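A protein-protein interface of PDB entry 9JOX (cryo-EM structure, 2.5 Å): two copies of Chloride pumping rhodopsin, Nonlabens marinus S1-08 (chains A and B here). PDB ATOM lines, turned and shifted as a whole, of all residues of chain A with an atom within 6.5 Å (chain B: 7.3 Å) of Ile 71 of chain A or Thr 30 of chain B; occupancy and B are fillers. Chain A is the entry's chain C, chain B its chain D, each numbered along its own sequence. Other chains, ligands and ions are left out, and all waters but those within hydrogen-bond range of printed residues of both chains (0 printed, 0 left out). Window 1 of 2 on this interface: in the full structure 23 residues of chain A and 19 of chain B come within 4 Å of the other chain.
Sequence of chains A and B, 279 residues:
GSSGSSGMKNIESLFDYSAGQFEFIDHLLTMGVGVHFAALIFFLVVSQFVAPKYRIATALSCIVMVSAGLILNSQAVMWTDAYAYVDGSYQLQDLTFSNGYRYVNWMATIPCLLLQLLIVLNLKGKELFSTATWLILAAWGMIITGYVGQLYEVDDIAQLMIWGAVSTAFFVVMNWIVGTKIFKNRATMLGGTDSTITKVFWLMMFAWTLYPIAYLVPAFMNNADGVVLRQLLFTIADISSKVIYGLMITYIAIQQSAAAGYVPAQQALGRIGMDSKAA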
ATOM      1  N   VAL A  33       2.380  27.026  15.924  1.00  0.00           N
ATOM      2  CA  VAL A  33       3.772  26.762  16.189  1.00  0.00           C
ATOM      3  C   VAL A  33       4.204  27.322  17.531  1.00  0.00           C
ATOM      4  O   VAL A  33       4.984  26.706  18.241  1.00  0.00           O
ATOM      5  CB  VAL A  33       4.713  27.315  15.119  1.00  0.00           C
ATOM      6  CG1 VAL A  33       6.172  27.154  15.526  1.00  0.00           C
ATOM      7  CG2 VAL A  33       4.425  26.649  13.785  1.00  0.00           C
ATOM      8  N   PHE A  37       5.656  25.445  21.186  1.00  0.00           N
ATOM      9  CA  PHE A  37       6.969  25.697  21.766  1.00  0.00           C
ATOM     10  C   PHE A  37       6.858  26.417  23.101  1.00  0.00           C
ATOM     11  O   PHE A  37       7.688  26.213  23.984  1.00  0.00           O
ATOM     12  CB  PHE A  37       7.918  26.394  20.812  1.00  0.00           C
ATOM     13  CG  PHE A  37       8.275  25.475  19.637  1.00  0.00           C
ATOM     14  CD1 PHE A  37       8.807  24.235  19.857  1.00  0.00           C
ATOM     15  CD2 PHE A  37       8.063  25.836  18.321  1.00  0.00           C
ATOM     16  CE1 PHE A  37       9.123  23.397  18.817  1.00  0.00           C
ATOM     17  CE2 PHE A  37       8.368  24.981  17.286  1.00  0.00           C
ATOM     18  CZ  PHE A  37       8.906  23.764  17.540  1.00  0.00           C
ATOM     19  N   VAL A  66       7.265  19.227  21.338  1.00  0.00           N
ATOM     20  CA  VAL A  66       8.351  19.479  20.386  1.00  0.00           C
ATOM     21  C   VAL A  66       8.012  18.872  19.020  1.00  0.00           C
ATOM     22  O   VAL A  66       8.208  19.486  17.987  1.00  0.00           O
ATOM     23  CB  VAL A  66       9.687  18.899  20.881  1.00  0.00           C
ATOM     24  CG1 VAL A  66      10.698  18.847  19.780  1.00  0.00           C
ATOM     25  CG2 VAL A  66      10.231  19.686  22.041  1.00  0.00           C
ATOM     26  N   SER A  67       7.557  17.634  19.028  1.00  0.00           N
ATOM     27  CA  SER A  67       7.218  16.937  17.806  1.00  0.00           C
ATOM     28  C   SER A  67       6.123  17.695  17.027  1.00  0.00           C
ATOM     29  O   SER A  67       6.314  18.049  15.876  1.00  0.00           O
ATOM     30  CB  SER A  67       6.790  15.548  18.166  1.00  0.00           C
ATOM     31  OG  SER A  67       6.076  14.951  17.109  1.00  0.00           O
ATOM     32  N   ALA A  68       4.981  17.953  17.657  1.00  0.00           N
ATOM     33  CA  ALA A  68       3.904  18.697  17.033  1.00  0.00           C
ATOM     34  C   ALA A  68       4.361  20.105  16.665  1.00  0.00           C
ATOM     35  O   ALA A  68       4.108  20.595  15.574  1.00  0.00           O
ATOM     36  CB  ALA A  68       2.693  18.759  17.933  1.00  0.00           C
ATOM     37  N   GLY A  69       5.077  20.778  17.522  1.00  0.00           N
ATOM     38  CA  GLY A  69       5.555  22.086  17.119  1.00  0.00           C
ATOM     39  C   GLY A  69       6.332  22.061  15.813  1.00  0.00           C
ATOM     40  O   GLY A  69       6.088  22.895  14.953  1.00  0.00           O
ATOM     41  N   LEU A  70       7.296  21.144  15.666  1.00  0.00           N
ATOM     42  CA  LEU A  70       8.107  21.122  14.455  1.00  0.00           C
ATOM     43  C   LEU A  70       7.305  20.729  13.196  1.00  0.00           C
ATOM     44  O   LEU A  70       7.611  21.206  12.127  1.00  0.00           O
ATOM     45  CB  LEU A  70       9.217  20.138  14.645  1.00  0.00           C
ATOM     46  CG  LEU A  70      10.331  20.522  15.579  1.00  0.00           C
ATOM     47  CD1 LEU A  70      11.298  19.393  15.764  1.00  0.00           C
ATOM     48  CD2 LEU A  70      10.955  21.661  14.983  1.00  0.00           C
ATOM     49  N   ILE A  71       6.273  19.909  13.307  1.00  0.00           N
ATOM     50  CA  ILE A  71       5.408  19.657  12.175  1.00  0.00           C
ATOM     51  C   ILE A  71       4.691  20.942  11.798  1.00  0.00           C
ATOM     52  O   ILE A  71       4.686  21.326  10.640  1.00  0.00           O
ATOM     53  CB  ILE A  71       4.396  18.505  12.395  1.00  0.00           C
ATOM     54  CG1 ILE A  71       5.075  17.213  12.320  1.00  0.00           C
ATOM     55  CG2 ILE A  71       3.297  18.496  11.343  1.00  0.00           C
ATOM     56  CD1 ILE A  71       5.690  16.943  10.966  1.00  0.00           C
ATOM     57  N   LEU A  72       4.035  21.578  12.746  1.00  0.00           N
ATOM     58  CA  LEU A  72       3.372  22.818  12.410  1.00  0.00           C
ATOM     59  C   LEU A  72       4.340  23.778  11.745  1.00  0.00           C
ATOM     60  O   LEU A  72       3.996  24.463  10.788  1.00  0.00           O
ATOM     61  CB  LEU A  72       2.691  23.451  13.616  1.00  0.00           C
ATOM     62  CG  LEU A  72       1.490  22.659  14.124  1.00  0.00           C
ATOM     63  CD1 LEU A  72       1.012  23.316  15.389  1.00  0.00           C
ATOM     64  CD2 LEU A  72       0.403  22.612  13.058  1.00  0.00           C
ATOM     65  N   ASN A  73       5.587  23.770  12.195  1.00  0.00           N
ATOM     66  CA  ASN A  73       6.460  24.770  11.635  1.00  0.00           C
ATOM     67  C   ASN A  73       6.754  24.488  10.152  1.00  0.00           C
ATOM     68  O   ASN A  73       6.818  25.372   9.321  1.00  0.00           O
ATOM     69  CB  ASN A  73       7.671  24.910  12.516  1.00  0.00           C
ATOM     70  CG  ASN A  73       8.585  25.932  11.935  1.00  0.00           C
ATOM     71  OD1 ASN A  73       8.213  27.099  11.833  1.00  0.00           O
ATOM     72  ND2 ASN A  73       9.700  25.474  11.431  1.00  0.00           N
ATOM     73  N   SER A  74       6.865  23.222   9.808  1.00  0.00           N
ATOM     74  CA  SER A  74       6.967  22.784   8.429  1.00  0.00           C
ATOM     75  C   SER A  74       5.729  23.148   7.625  1.00  0.00           C
ATOM     76  O   SER A  74       5.878  23.722   6.561  1.00  0.00           O
ATOM     77  CB  SER A  74       7.202  21.297   8.333  1.00  0.00           C
ATOM     78  OG  SER A  74       8.562  21.033   8.605  1.00  0.00           O
ATOM     79  N   GLN A  75       4.530  22.750   8.092  1.00  0.00           N
ATOM     80  CA  GLN A  75       3.342  23.086   7.342  1.00  0.00           C
ATOM     81  C   GLN A  75       3.353  24.587   7.041  1.00  0.00           C
ATOM     82  O   GLN A  75       3.058  25.004   5.939  1.00  0.00           O
ATOM     83  CB  GLN A  75       2.054  22.819   8.062  1.00  0.00           C
ATOM     84  CG  GLN A  75       1.790  21.341   8.164  1.00  0.00           C
ATOM     85  CD  GLN A  75       1.277  20.804   6.867  1.00  0.00           C
ATOM     86  OE1 GLN A  75       2.016  20.770   5.875  1.00  0.00           O
ATOM     87  NE2 GLN A  75       0.010  20.403   6.871  1.00  0.00           N
ATOM     88  N   ALA A  76       3.792  25.385   7.990  1.00  0.00           N
ATOM     89  CA  ALA A  76       3.600  26.803   7.855  1.00  0.00           C
ATOM     90  C   ALA A  76       4.520  27.342   6.785  1.00  0.00           C
ATOM     91  O   ALA A  76       4.142  28.248   6.049  1.00  0.00           O
ATOM     92  CB  ALA A  76       3.870  27.494   9.187  1.00  0.00           C
ATOM     93  N   TYR A 101       1.731  15.311   6.394  1.00  0.00           N
ATOM     94  CA  TYR A 101       2.674  15.574   7.465  1.00  0.00           C
ATOM     95  C   TYR A 101       2.073  15.276   8.843  1.00  0.00           C
ATOM     96  O   TYR A 101       2.703  14.653   9.683  1.00  0.00           O
ATOM     97  CB  TYR A 101       3.139  17.028   7.479  1.00  0.00           C
ATOM     98  CG  TYR A 101       3.886  17.321   6.204  1.00  0.00           C
ATOM     99  CD1 TYR A 101       3.207  17.697   5.058  1.00  0.00           C
ATOM    100  CD2 TYR A 101       5.252  17.094   6.114  1.00  0.00           C
ATOM    101  CE1 TYR A 101       3.875  17.874   3.856  1.00  0.00           C
ATOM    102  CE2 TYR A 101       5.933  17.273   4.922  1.00  0.00           C
ATOM    103  CZ  TYR A 101       5.238  17.675   3.794  1.00  0.00           C
ATOM    104  OH  TYR A 101       5.863  17.910   2.611  1.00  0.00           O
ATOM    105  N   ARG A 102       0.853  15.722   9.085  1.00  0.00           N
ATOM    106  CA  ARG A 102       0.235  15.494  10.368  1.00  0.00           C
ATOM    107  C   ARG A 102       0.016  14.006  10.578  1.00  0.00           C
ATOM    108  O   ARG A 102       0.407  13.463  11.600  1.00  0.00           O
ATOM    109  CB  ARG A 102      -1.068  16.261  10.448  1.00  0.00           C
ATOM    110  CG  ARG A 102      -0.902  17.770  10.388  1.00  0.00           C
ATOM    111  CD  ARG A 102      -2.383  18.237  10.179  1.00  0.00           C
ATOM    112  NE  ARG A 102      -2.451  19.698  10.206  1.00  0.00           N
ATOM    113  CZ  ARG A 102      -2.343  20.412  11.308  1.00  0.00           C
ATOM    114  NH1 ARG A 102      -2.344  19.841  12.506  1.00  0.00           N
ATOM    115  NH2 ARG A 102      -2.428  21.692  11.192  1.00  0.00           N
ATOM    116  N   ASN A 105       3.003  12.154  11.641  1.00  0.00           N
ATOM    117  CA  ASN A 105       3.408  12.532  12.982  1.00  0.00           C
ATOM    118  C   ASN A 105       2.551  11.932  14.131  1.00  0.00           C
ATOM    119  O   ASN A 105       3.068  11.639  15.195  1.00  0.00           O
ATOM    120  CB  ASN A 105       3.425  14.032  13.093  1.00  0.00           C
ATOM    121  CG  ASN A 105       4.394  14.395  14.166  1.00  0.00           C
ATOM    122  OD1 ASN A 105       5.593  14.119  14.001  1.00  0.00           O
ATOM    123  ND2 ASN A 105       3.882  15.009  15.230  1.00  0.00           N
ATOM    124  N   GLU B  23       5.404  13.239  -2.010  1.00  0.00           N
ATOM    125  CA  GLU B  23       4.941  13.797  -0.738  1.00  0.00           C
ATOM    126  C   GLU B  23       5.166  12.791   0.405  1.00  0.00           C
ATOM    127  O   GLU B  23       5.573  13.173   1.490  1.00  0.00           O
ATOM    128  CB  GLU B  23       3.497  14.257  -0.791  1.00  0.00           C
ATOM    129  CG  GLU B  23       3.247  15.477  -1.660  1.00  0.00           C
ATOM    130  CD  GLU B  23       1.757  15.708  -1.962  1.00  0.00           C
ATOM    131  OE1 GLU B  23       0.914  14.783  -1.768  1.00  0.00           O
ATOM    132  OE2 GLU B  23       1.415  16.850  -2.372  1.00  0.00           O
ATOM    133  N   PHE B  24       4.975  11.495   0.129  1.00  0.00           N
ATOM    134  CA  PHE B  24       5.194  10.446   1.107  1.00  0.00           C
ATOM    135  C   PHE B  24       6.611  10.534   1.687  1.00  0.00           C
ATOM    136  O   PHE B  24       6.811  10.634   2.904  1.00  0.00           O
ATOM    137  CB  PHE B  24       4.997   9.073   0.467  1.00  0.00           C
ATOM    138  CG  PHE B  24       5.004   7.893   1.420  1.00  0.00           C
ATOM    139  CD1 PHE B  24       4.260   7.933   2.589  1.00  0.00           C
ATOM    140  CD2 PHE B  24       5.837   6.795   1.186  1.00  0.00           C
ATOM    141  CE1 PHE B  24       4.341   6.897   3.522  1.00  0.00           C
ATOM    142  CE2 PHE B  24       5.911   5.764   2.106  1.00  0.00           C
ATOM    143  CZ  PHE B  24       5.174   5.826   3.279  1.00  0.00           C
ATOM    144  N   ILE B  25       7.594  10.549   0.800  1.00  0.00           N
ATOM    145  CA  ILE B  25       8.972  10.658   1.242  1.00  0.00           C
ATOM    146  C   ILE B  25       9.186  11.936   2.052  1.00  0.00           C
ATOM    147  O   ILE B  25       9.823  11.878   3.091  1.00  0.00           O
ATOM    148  CB  ILE B  25       9.921  10.577   0.041  1.00  0.00           C
ATOM    149  CG1 ILE B  25       9.990   9.155  -0.498  1.00  0.00           C
ATOM    150  CG2 ILE B  25      11.284  11.101   0.440  1.00  0.00           C
ATOM    151  CD1 ILE B  25      10.656   9.073  -1.847  1.00  0.00           C
ATOM    152  N   ASP B  26       8.599  13.066   1.664  1.00  0.00           N
ATOM    153  CA  ASP B  26       8.776  14.256   2.484  1.00  0.00           C
ATOM    154  C   ASP B  26       8.114  14.082   3.861  1.00  0.00           C
ATOM    155  O   ASP B  26       8.632  14.586   4.860  1.00  0.00           O
ATOM    156  CB  ASP B  26       8.282  15.526   1.807  1.00  0.00           C
ATOM    157  CG  ASP B  26       8.886  16.794   2.404  1.00  0.00           C
ATOM    158  OD1 ASP B  26      10.050  16.737   2.901  1.00  0.00           O
ATOM    159  OD2 ASP B  26       8.191  17.843   2.403  1.00  0.00           O
ATOM    160  N   HIS B  27       6.988  13.368   3.922  1.00  0.00           N
ATOM    161  CA  HIS B  27       6.340  13.076   5.184  1.00  0.00           C
ATOM    162  C   HIS B  27       7.241  12.211   6.069  1.00  0.00           C
ATOM    163  O   HIS B  27       7.400  12.511   7.246  1.00  0.00           O
ATOM    164  CB  HIS B  27       4.971  12.405   5.013  1.00  0.00           C
ATOM    165  CG  HIS B  27       3.994  13.180   4.221  1.00  0.00           C
ATOM    166  ND1 HIS B  27       4.032  14.555   4.011  1.00  0.00           N
ATOM    167  CD2 HIS B  27       2.944  12.696   3.518  1.00  0.00           C
ATOM    168  CE1 HIS B  27       3.003  14.877   3.206  1.00  0.00           C
ATOM    169  NE2 HIS B  27       2.298  13.783   2.937  1.00  0.00           N
ATOM    170  N   LEU B  28       7.836  11.139   5.541  1.00  0.00           N
ATOM    171  CA  LEU B  28       8.747  10.347   6.364  1.00  0.00           C
ATOM    172  C   LEU B  28       9.948  11.155   6.862  1.00  0.00           C
ATOM    173  O   LEU B  28      10.225  11.164   8.051  1.00  0.00           O
ATOM    174  CB  LEU B  28       9.214   9.156   5.567  1.00  0.00           C
ATOM    175  CG  LEU B  28       8.147   8.115   5.243  1.00  0.00           C
ATOM    176  CD1 LEU B  28       8.849   7.099   4.352  1.00  0.00           C
ATOM    177  CD2 LEU B  28       7.658   7.514   6.522  1.00  0.00           C
ATOM    178  N   LEU B  29      10.627  11.875   5.994  1.00  0.00           N
ATOM    179  CA  LEU B  29      11.783  12.630   6.444  1.00  0.00           C
ATOM    180  C   LEU B  29      11.368  13.629   7.500  1.00  0.00           C
ATOM    181  O   LEU B  29      12.048  13.782   8.491  1.00  0.00           O
ATOM    182  CB  LEU B  29      12.560  13.320   5.317  1.00  0.00           C
ATOM    183  CG  LEU B  29      13.065  12.401   4.187  1.00  0.00           C
ATOM    184  CD1 LEU B  29      13.503  13.186   2.965  1.00  0.00           C
ATOM    185  CD2 LEU B  29      14.205  11.649   4.725  1.00  0.00           C
ATOM    186  N   THR B  30      10.236  14.297   7.341  1.00  0.00           N
ATOM    187  CA  THR B  30       9.914  15.343   8.299  1.00  0.00           C
ATOM    188  C   THR B  30       9.642  14.764   9.691  1.00  0.00           C
ATOM    189  O   THR B  30      10.033  15.323  10.727  1.00  0.00           O
ATOM    190  CB  THR B  30       8.773  16.165   7.743  1.00  0.00           C
ATOM    191  OG1 THR B  30       9.295  16.760   6.546  1.00  0.00           O
ATOM    192  CG2 THR B  30       8.409  17.314   8.661  1.00  0.00           C
ATOM    193  N   MET B  31       9.049  13.596   9.729  1.00  0.00           N
ATOM    194  CA  MET B  31       8.678  13.009  10.998  1.00  0.00           C
ATOM    195  C   MET B  31       9.936  12.549  11.737  1.00  0.00           C
ATOM    196  O   MET B  31      10.117  12.871  12.883  1.00  0.00           O
ATOM    197  CB  MET B  31       7.710  11.855  10.750  1.00  0.00           C
ATOM    198  CG  MET B  31       7.197  11.212  11.981  1.00  0.00           C
ATOM    199  SD  MET B  31       8.135   9.714  12.288  1.00  0.00           S
ATOM    200  CE  MET B  31       7.684   8.794  10.808  1.00  0.00           C
ATOM    201  N   GLY B  32      10.815  11.853  11.046  1.00  0.00           N
ATOM    202  CA  GLY B  32      12.125  11.515  11.572  1.00  0.00           C
ATOM    203  C   GLY B  32      12.820  12.666  12.290  1.00  0.00           C
ATOM    204  O   GLY B  32      13.249  12.517  13.419  1.00  0.00           O
ATOM    205  N   VAL B  33      12.843  13.842  11.703  1.00  0.00           N
ATOM    206  CA  VAL B  33      13.516  14.930  12.372  1.00  0.00           C
ATOM    207  C   VAL B  33      12.925  15.177  13.751  1.00  0.00           C
ATOM    208  O   VAL B  33      13.623  15.505  14.689  1.00  0.00           O
ATOM    209  CB  VAL B  33      13.433  16.253  11.597  1.00  0.00           C
ATOM    210  CG1 VAL B  33      14.052  17.379  12.452  1.00  0.00           C
ATOM    211  CG2 VAL B  33      14.129  16.139  10.242  1.00  0.00           C
ATOM    212  N   GLY B  34      11.612  15.122  13.869  1.00  0.00           N
ATOM    213  CA  GLY B  34      10.972  15.579  15.086  1.00  0.00           C
ATOM    214  C   GLY B  34      10.965  14.523  16.174  1.00  0.00           C
ATOM    215  O   GLY B  34      11.158  14.851  17.356  1.00  0.00           O
ATOM    216  N   VAL B  35      10.844  13.256  15.780  1.00  0.00           N
ATOM    217  CA  VAL B  35      11.030  12.188  16.745  1.00  0.00           C
ATOM    218  C   VAL B  35      12.418  12.286  17.392  1.00  0.00           C
ATOM    219  O   VAL B  35      12.536  12.198  18.599  1.00  0.00           O
ATOM    220  CB  VAL B  35      10.735  10.822  16.134  1.00  0.00           C
ATOM    221  CG1 VAL B  35      11.053   9.705  17.079  1.00  0.00           C
ATOM    222  CG2 VAL B  35       9.259  10.716  15.847  1.00  0.00           C
ATOM    223  N   LEU B  72      18.913  14.303   9.484  1.00  0.00           N
ATOM    224  CA  LEU B  72      17.609  14.192   8.874  1.00  0.00           C
ATOM    225  C   LEU B  72      17.129  15.568   8.445  1.00  0.00           C
ATOM    226  O   LEU B  72      16.519  15.734   7.400  1.00  0.00           O
ATOM    227  CB  LEU B  72      16.616  13.503   9.777  1.00  0.00           C
ATOM    228  CG  LEU B  72      16.909  12.005   9.949  1.00  0.00           C
ATOM    229  CD1 LEU B  72      15.935  11.403  10.947  1.00  0.00           C
ATOM    230  CD2 LEU B  72      16.810  11.286   8.656  1.00  0.00           C
ATOM    231  N   ALA B  76      16.036  16.525   4.629  1.00  0.00           N
ATOM    232  CA  ALA B  76      14.657  16.876   4.317  1.00  0.00           C
ATOM    233  C   ALA B  76      14.613  18.188   3.549  1.00  0.00           C
ATOM    234  O   ALA B  76      13.803  18.345   2.660  1.00  0.00           O
ATOM    235  CB  ALA B  76      13.831  16.978   5.555  1.00  0.00           C
ATOM    236  N   VAL B  77      15.483  19.126   3.897  1.00  0.00           N
ATOM    237  CA  VAL B  77      15.609  20.344   3.118  1.00  0.00           C
ATOM    238  C   VAL B  77      16.131  20.098   1.691  1.00  0.00           C
ATOM    239  O   VAL B  77      15.715  20.739   0.746  1.00  0.00           O
ATOM    240  CB  VAL B  77      16.576  21.261   3.854  1.00  0.00           C
ATOM    241  CG1 VAL B  77      16.978  22.405   2.960  1.00  0.00           C
ATOM    242  CG2 VAL B  77      15.968  21.775   5.120  1.00  0.00           C
ATOM    243  N   THR B 235      13.730   5.040   7.475  1.00  0.00           N
ATOM    244  CA  THR B 235      13.026   5.724   8.533  1.00  0.00           C
ATOM    245  C   THR B 235      12.775   4.784   9.704  1.00  0.00           C
ATOM    246  O   THR B 235      13.052   5.123  10.857  1.00  0.00           O
ATOM    247  CB  THR B 235      11.743   6.377   8.035  1.00  0.00           C
ATOM    248  OG1 THR B 235      12.290   7.366   7.170  1.00  0.00           O
ATOM    249  CG2 THR B 235      10.941   7.035   9.156  1.00  0.00           C
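The side-chain hydroxyl (OH) of Tyr 101 of chain A sits close to the side-chain carboxylate (OD2) of Asp 26 of chain B, 2.3 Å away.
N of Tyr 101 of chain A sits close to ND1 of His 27 of chain B, 3.4 Å away.
Ile 71 of chain A touches just one residue of chain B: Thr 30.
Of chain A, only Ile 71, Ser 74 and Tyr 101 come within 4 Å of Thr 30 of chain B.
Of the printed residues of chain A, His 27 of chain B touches Tyr 101.
Of the printed residues of chain A, Gly 34 of chain B touches Leu 70 (3.9 Å).
Of the printed residues of chain B, Leu 70 of chain A touches Gly 34.
Printed residues of chain B within 4 Å of Asn 105 of chain A: Met 31.
Val 33 of chain B touches none of the printed residues of chain A.
The nearest printed residue of chain A that does not touch Asp 26 of chain B is Ser 74 of chain A (6.9 Å).
Among the printed residues, merely in contact across the chains: Ile 71 of chain A with Thr 30 of chain B (3.6 Å), Ser 74 of chain A with Thr 30 of chain B (3.7 Å), Tyr 101 of chain A with Thr 30 of chain B (3.8 Å), Asn 105 of chain A with Met 31 of chain B (3.9 Å) and Leu 70 of chain A with Gly 34 of chain B (3.9 Å).
3 positions are printed for both chains.
The backbone carbonyl oxygen (O) of Glu 23 of chain B sits close to a ring nitrogen (ND1) of His 27 of chain B (3.3 Å).
The side-chain amide nitrogen of Asn 105 of chain A is in hydrogen-bond range of the side-chain hydroxyl of Ser 67 of chain A (2.9 Å).
The backbone carbonyl oxygen (O) of Asp 26 of chain B sits at hydrogen-bond distance from the side-chain hydroxyl (OG1) of Thr 30 of chain B (2.8 Å).
Of the 17 printed residues of chain B, 5 touch a printed residue of chain A.
Hydrophobic or aromatic side chains of chain B within 4 Å of the printed part of chain A: His 27 and Met 31.
Among the printed residues, 7 pairs touch across the chains.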
